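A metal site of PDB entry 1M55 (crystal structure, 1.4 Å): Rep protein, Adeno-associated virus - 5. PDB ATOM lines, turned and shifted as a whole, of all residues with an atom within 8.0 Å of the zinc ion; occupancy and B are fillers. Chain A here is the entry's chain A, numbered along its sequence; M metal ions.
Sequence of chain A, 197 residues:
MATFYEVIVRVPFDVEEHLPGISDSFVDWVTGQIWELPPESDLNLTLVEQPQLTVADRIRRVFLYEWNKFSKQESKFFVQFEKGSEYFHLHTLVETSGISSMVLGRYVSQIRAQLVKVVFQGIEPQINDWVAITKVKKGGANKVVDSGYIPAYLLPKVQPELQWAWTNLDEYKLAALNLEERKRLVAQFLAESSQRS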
ATOM      1  N   GLU A   6       3.602  23.043  16.313  1.00  0.00           N
ATOM      2  CA  GLU A   6       3.354  22.930  17.740  1.00  0.00           C
ATOM      3  C   GLU A   6       2.494  21.725  18.029  1.00  0.00           C
ATOM      4  O   GLU A   6       1.434  21.548  17.423  1.00  0.00           O
ATOM      5  CB  GLU A   6       2.669  24.166  18.345  1.00  0.00           C
ATOM      6  CG  GLU A   6       2.437  23.988  19.868  1.00  0.00           C
ATOM      7  CD  GLU A   6       1.641  25.108  20.503  1.00  0.00           C
ATOM      8  OE1 GLU A   6       0.488  25.334  20.077  1.00  0.00           O
ATOM      9  OE2 GLU A   6       2.148  25.737  21.454  1.00  0.00           O
ATOM     10  N   ILE A   8       0.845  19.793  21.322  1.00  0.00           N
ATOM     11  CA  ILE A   8       0.619  19.869  22.752  1.00  0.00           C
ATOM     12  C   ILE A   8       0.369  18.461  23.267  1.00  0.00           C
ATOM     13  O   ILE A   8      -0.473  17.730  22.730  1.00  0.00           O
ATOM     14  CB  ILE A   8      -0.549  20.814  23.117  1.00  0.00           C
ATOM     15  CG1 ILE A   8      -0.180  22.250  22.754  1.00  0.00           C
ATOM     16  CG2 ILE A   8      -0.855  20.715  24.621  1.00  0.00           C
ATOM     17  CD1 ILE A   8      -1.288  23.265  23.011  1.00  0.00           C
ATOM     18  N   GLN A  80       7.998  23.666  26.480  1.00  0.00           N
ATOM     19  CA  GLN A  80       7.651  24.227  27.780  1.00  0.00           C
ATOM     20  C   GLN A  80       6.602  23.369  28.487  1.00  0.00           C
ATOM     21  O   GLN A  80       5.556  23.056  27.908  1.00  0.00           O
ATOM     22  CB  GLN A  80       7.171  25.672  27.641  1.00  0.00           C
ATOM     23  CG  GLN A  80       6.853  26.338  28.969  1.00  0.00           C
ATOM     24  CD  GLN A  80       6.886  27.846  28.870  1.00  0.00           C
ATOM     25  OE1 GLN A  80       7.947  28.437  28.749  1.00  0.00           O
ATOM     26  NE2 GLN A  80       5.719  28.473  28.908  1.00  0.00           N
ATOM     27  N   PHE A  81       6.923  22.955  29.706  1.00  0.00           N
ATOM     28  CA  PHE A  81       6.034  22.140  30.534  1.00  0.00           C
ATOM     29  C   PHE A  81       5.226  23.081  31.433  1.00  0.00           C
ATOM     30  O   PHE A  81       5.790  23.920  32.152  1.00  0.00           O
ATOM     31  CB  PHE A  81       6.871  21.171  31.385  1.00  0.00           C
ATOM     32  CG  PHE A  81       6.046  20.215  32.209  1.00  0.00           C
ATOM     33  CD1 PHE A  81       6.395  19.935  33.525  1.00  0.00           C
ATOM     34  CD2 PHE A  81       4.919  19.598  31.667  1.00  0.00           C
ATOM     35  CE1 PHE A  81       5.630  19.057  34.299  1.00  0.00           C
ATOM     36  CE2 PHE A  81       4.144  18.728  32.440  1.00  0.00           C
ATOM     37  CZ  PHE A  81       4.505  18.454  33.757  1.00  0.00           C
ATOM     38  N   GLU A  82       3.906  22.925  31.399  1.00  0.00           N
ATOM     39  CA  GLU A  82       3.017  23.786  32.179  1.00  0.00           C
ATOM     40  C   GLU A  82       1.953  23.016  32.965  1.00  0.00           C
ATOM     41  O   GLU A  82       1.594  21.886  32.615  1.00  0.00           O
ATOM     42  CB  GLU A  82       2.280  24.765  31.259  1.00  0.00           C
ATOM     43  CG  GLU A  82       3.179  25.751  30.532  1.00  0.00           C
ATOM     44  CD  GLU A  82       2.428  26.602  29.516  1.00  0.00           C
ATOM     45  OE1 GLU A  82       1.179  26.516  29.450  1.00  0.00           O
ATOM     46  OE2 GLU A  82       3.083  27.356  28.778  1.00  0.00           O
ATOM     47  N   LYS A  83       1.470  23.651  34.027  1.00  0.00           N
ATOM     48  CA  LYS A  83       0.417  23.108  34.866  1.00  0.00           C
ATOM     49  C   LYS A  83      -0.812  23.924  34.460  1.00  0.00           C
ATOM     50  O   LYS A  83      -0.966  25.076  34.890  1.00  0.00           O
ATOM     51  CB  LYS A  83       0.752  23.315  36.343  1.00  0.00           C
ATOM     52  CG  LYS A  83      -0.270  22.772  37.311  1.00  0.00           C
ATOM     53  CD  LYS A  83       0.196  22.987  38.750  1.00  0.00           C
ATOM     54  CE  LYS A  83      -0.661  22.200  39.741  1.00  0.00           C
ATOM     55  NZ  LYS A  83      -2.095  22.617  39.708  1.00  0.00           N
ATOM     56  N   GLY A  84      -1.610  23.381  33.557  1.00  0.00           N
ATOM     57  CA  GLY A  84      -2.802  24.072  33.099  1.00  0.00           C
ATOM     58  C   GLY A  84      -3.956  23.954  34.082  1.00  0.00           C
ATOM     59  O   GLY A  84      -3.816  23.341  35.155  1.00  0.00           O
ATOM     60  N   SER A  85      -5.098  24.506  33.712  1.00  0.00           N
ATOM     61  CA  SER A  85      -6.271  24.444  34.577  1.00  0.00           C
ATOM     62  C   SER A  85      -6.800  23.013  34.698  1.00  0.00           C
ATOM     63  O   SER A  85      -7.283  22.610  35.751  1.00  0.00           O
ATOM     64  CB  SER A  85      -7.370  25.366  34.039  1.00  0.00           C
ATOM     65  OG  SER A  85      -7.489  25.224  32.633  1.00  0.00           O
ATOM     66  N   TYR A  87      -4.970  20.114  32.794  1.00  0.00           N
ATOM     67  CA  TYR A  87      -3.906  19.133  32.631  1.00  0.00           C
ATOM     68  C   TYR A  87      -2.501  19.700  32.655  1.00  0.00           C
ATOM     69  O   TYR A  87      -2.283  20.866  32.323  1.00  0.00           O
ATOM     70  CB  TYR A  87      -4.023  18.452  31.268  1.00  0.00           C
ATOM     71  CG  TYR A  87      -5.339  17.793  30.962  1.00  0.00           C
ATOM     72  CD1 TYR A  87      -6.340  18.483  30.298  1.00  0.00           C
ATOM     73  CD2 TYR A  87      -5.583  16.474  31.337  1.00  0.00           C
ATOM     74  CE1 TYR A  87      -7.554  17.871  29.998  1.00  0.00           C
ATOM     75  CE2 TYR A  87      -6.790  15.847  31.033  1.00  0.00           C
ATOM     76  CZ  TYR A  87      -7.768  16.555  30.364  1.00  0.00           C
ATOM     77  OH  TYR A  87      -8.963  15.956  30.053  1.00  0.00           O
ATOM     78  N   PHE A  88      -1.562  18.855  33.053  1.00  0.00           N
ATOM     79  CA  PHE A  88      -0.152  19.221  32.984  1.00  0.00           C
ATOM     80  C   PHE A  88       0.062  18.939  31.495  1.00  0.00           C
ATOM     81  O   PHE A  88      -0.449  17.941  30.970  1.00  0.00           O
ATOM     82  CB  PHE A  88       0.696  18.265  33.813  1.00  0.00           C
ATOM     83  CG  PHE A  88       0.691  18.569  35.275  1.00  0.00           C
ATOM     84  CD1 PHE A  88      -0.301  18.063  36.111  1.00  0.00           C
ATOM     85  CD2 PHE A  88       1.672  19.386  35.832  1.00  0.00           C
ATOM     86  CE1 PHE A  88      -0.308  18.351  37.476  1.00  0.00           C
ATOM     87  CE2 PHE A  88       1.675  19.688  37.191  1.00  0.00           C
ATOM     88  CZ  PHE A  88       0.685  19.160  38.016  1.00  0.00           C
ATOM     89  N   HIS A  89       0.779  19.808  30.799  1.00  0.00           N
ATOM     90  CA  HIS A  89       0.966  19.593  29.370  1.00  0.00           C
ATOM     91  C   HIS A  89       2.231  20.228  28.862  1.00  0.00           C
ATOM     92  O   HIS A  89       2.813  21.107  29.505  1.00  0.00           O
ATOM     93  CB  HIS A  89      -0.247  20.131  28.596  1.00  0.00           C
ATOM     94  CG  HIS A  89      -0.495  21.602  28.815  1.00  0.00           C
ATOM     95  ND1 HIS A  89      -1.136  22.118  29.910  1.00  0.00           N
ATOM     96  CD2 HIS A  89      -0.105  22.666  28.068  1.00  0.00           C
ATOM     97  CE1 HIS A  89      -1.116  23.450  29.820  1.00  0.00           C
ATOM     98  NE2 HIS A  89      -0.508  23.825  28.706  1.00  0.00           N
ATOM     99  N   LEU A  90       2.659  19.760  27.699  1.00  0.00           N
ATOM    100  CA  LEU A  90       3.864  20.271  27.057  1.00  0.00           C
ATOM    101  C   LEU A  90       3.560  20.980  25.756  1.00  0.00           C
ATOM    102  O   LEU A  90       2.804  20.456  24.919  1.00  0.00           O
ATOM    103  CB  LEU A  90       4.799  19.100  26.716  1.00  0.00           C
ATOM    104  CG  LEU A  90       5.478  18.308  27.836  1.00  0.00           C
ATOM    105  CD1 LEU A  90       5.845  16.920  27.334  1.00  0.00           C
ATOM    106  CD2 LEU A  90       6.691  19.066  28.340  1.00  0.00           C
ATOM    107  N   HIS A  91       4.062  22.200  25.610  1.00  0.00           N
ATOM    108  CA  HIS A  91       3.943  22.943  24.356  1.00  0.00           C
ATOM    109  C   HIS A  91       5.232  22.506  23.674  1.00  0.00           C
ATOM    110  O   HIS A  91       6.324  22.869  24.127  1.00  0.00           O
ATOM    111  CB  HIS A  91       3.957  24.452  24.574  1.00  0.00           C
ATOM    112  CG  HIS A  91       2.668  24.992  25.103  1.00  0.00           C
ATOM    113  ND1 HIS A  91       1.675  25.529  24.304  1.00  0.00           N
ATOM    114  CD2 HIS A  91       2.198  25.047  26.367  1.00  0.00           C
ATOM    115  CE1 HIS A  91       0.662  25.891  25.106  1.00  0.00           C
ATOM    116  NE2 HIS A  91       0.932  25.618  26.370  1.00  0.00           N
ATOM    117  N   TYR A 149       6.845  33.567  18.485  1.00  0.00           N
ATOM    118  CA  TYR A 149       5.814  32.929  19.298  1.00  0.00           C
ATOM    119  C   TYR A 149       6.356  32.589  20.693  1.00  0.00           C
ATOM    120  O   TYR A 149       5.622  32.607  21.684  1.00  0.00           O
ATOM    121  CB  TYR A 149       5.335  31.662  18.585  1.00  0.00           C
ATOM    122  CG  TYR A 149       4.254  30.857  19.289  1.00  0.00           C
ATOM    123  CD1 TYR A 149       2.910  31.191  19.148  1.00  0.00           C
ATOM    124  CD2 TYR A 149       4.581  29.708  20.012  1.00  0.00           C
ATOM    125  CE1 TYR A 149       1.907  30.404  19.707  1.00  0.00           C
ATOM    126  CE2 TYR A 149       3.579  28.900  20.577  1.00  0.00           C
ATOM    127  CZ  TYR A 149       2.251  29.254  20.419  1.00  0.00           C
ATOM    128  OH  TYR A 149       1.253  28.458  20.949  1.00  0.00           O
ATOM    129  N   TYR A 153       4.342  34.401  23.607  1.00  0.00           N
ATOM    130  CA  TYR A 153       3.382  33.555  24.286  1.00  0.00           C
ATOM    131  C   TYR A 153       3.881  32.617  25.368  1.00  0.00           C
ATOM    132  O   TYR A 153       3.238  32.464  26.404  1.00  0.00           O
ATOM    133  CB  TYR A 153       2.651  32.768  23.207  1.00  0.00           C
ATOM    134  CG  TYR A 153       1.446  31.977  23.648  1.00  0.00           C
ATOM    135  CD1 TYR A 153       0.325  32.608  24.186  1.00  0.00           C
ATOM    136  CD2 TYR A 153       1.394  30.600  23.441  1.00  0.00           C
ATOM    137  CE1 TYR A 153      -0.829  31.895  24.484  1.00  0.00           C
ATOM    138  CE2 TYR A 153       0.243  29.879  23.728  1.00  0.00           C
ATOM    139  CZ  TYR A 153      -0.858  30.522  24.238  1.00  0.00           C
ATOM    140  OH  TYR A 153      -2.011  29.814  24.460  1.00  0.00           O
ATOM    141  N   LEU A 154       5.019  31.961  25.132  1.00  0.00           N
ATOM    142  CA  LEU A 154       5.536  31.012  26.111  1.00  0.00           C
ATOM    143  C   LEU A 154       6.382  31.611  27.237  1.00  0.00           C
ATOM    144  O   LEU A 154       6.165  31.291  28.405  1.00  0.00           O
ATOM    145  CB  LEU A 154       6.318  29.900  25.411  1.00  0.00           C
ATOM    146  CG  LEU A 154       5.517  29.106  24.375  1.00  0.00           C
ATOM    147  CD1 LEU A 154       6.413  28.020  23.780  1.00  0.00           C
ATOM    148  CD2 LEU A 154       4.278  28.485  25.000  1.00  0.00           C
ATOM    149  N   LYS A 157       4.851  33.125  30.765  1.00  0.00           N
ATOM    150  CA  LYS A 157       4.312  32.280  31.825  1.00  0.00           C
ATOM    151  C   LYS A 157       5.175  32.311  33.082  1.00  0.00           C
ATOM    152  O   LYS A 157       6.397  32.289  32.987  1.00  0.00           O
ATOM    153  CB  LYS A 157       4.127  30.832  31.357  1.00  0.00           C
ATOM    154  CG  LYS A 157       2.807  30.543  30.631  1.00  0.00           C
ATOM    155  CD  LYS A 157       2.812  31.035  29.201  1.00  0.00           C
ATOM    156  CE  LYS A 157       1.451  30.858  28.544  1.00  0.00           C
ATOM    157  NZ  LYS A 157       1.003  29.437  28.526  1.00  0.00           N
ATOM    158  N   GLU A 161       2.156  28.055  36.836  1.00  0.00           N
ATOM    159  CA  GLU A 161       1.780  27.598  35.490  1.00  0.00           C
ATOM    160  C   GLU A 161       3.026  27.087  34.790  1.00  0.00           C
ATOM    161  O   GLU A 161       3.017  26.004  34.196  1.00  0.00           O
ATOM    162  CB  GLU A 161       1.149  28.724  34.661  1.00  0.00           C
ATOM    163  CG  GLU A 161       0.714  28.230  33.283  1.00  0.00           C
ATOM    164  CD  GLU A 161       0.072  29.286  32.408  1.00  0.00           C
ATOM    165  OE1 GLU A 161      -0.161  30.419  32.885  1.00  0.00           O
ATOM    166  OE2 GLU A 161      -0.208  28.972  31.233  1.00  0.00           O
HETATM  167 ZN    ZN M   1      -0.134  25.731  28.054  1.00  0.00          ZN
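O of Gln 80 sits at hydrogen-bond distance from N of His 91 (2.9 Å).
ND1 of His 91 lies within hydrogen-bond range of OE2 of Glu 6 (2.9 Å).
A ring nitrogen (ND1) of His 89 lies within hydrogen-bond range of the backbone carbonyl oxygen (O) of Tyr 87 (3.0 Å).
OE2 of Glu 82 is in salt-bridge range of NZ of Lys 157, 3.0 Å away.
NE2 of Gln 80 is in hydrogen-bond range of OE2 of Glu 82, at 2.9 Å.
The side-chain amino group (NZ) of Lys 157 is in salt-bridge range of the side-chain carboxylate (OE2) of Glu 161, at 3.0 Å.
Merely in contact with the zinc ion: Lys 157.
Four residues have an atom within 4 Å of the zinc ion: Glu 82, His 89, His 91 and Lys 157.
The nearest printed residue that does not touch the zinc ion is Glu 161 (4.5 Å).
The zinc ion is bound by NE2 of His 91 (2.0 Å), NE2 of His 89 (2.0 Å) and OE1 of Glu 82 (2.1 Å).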
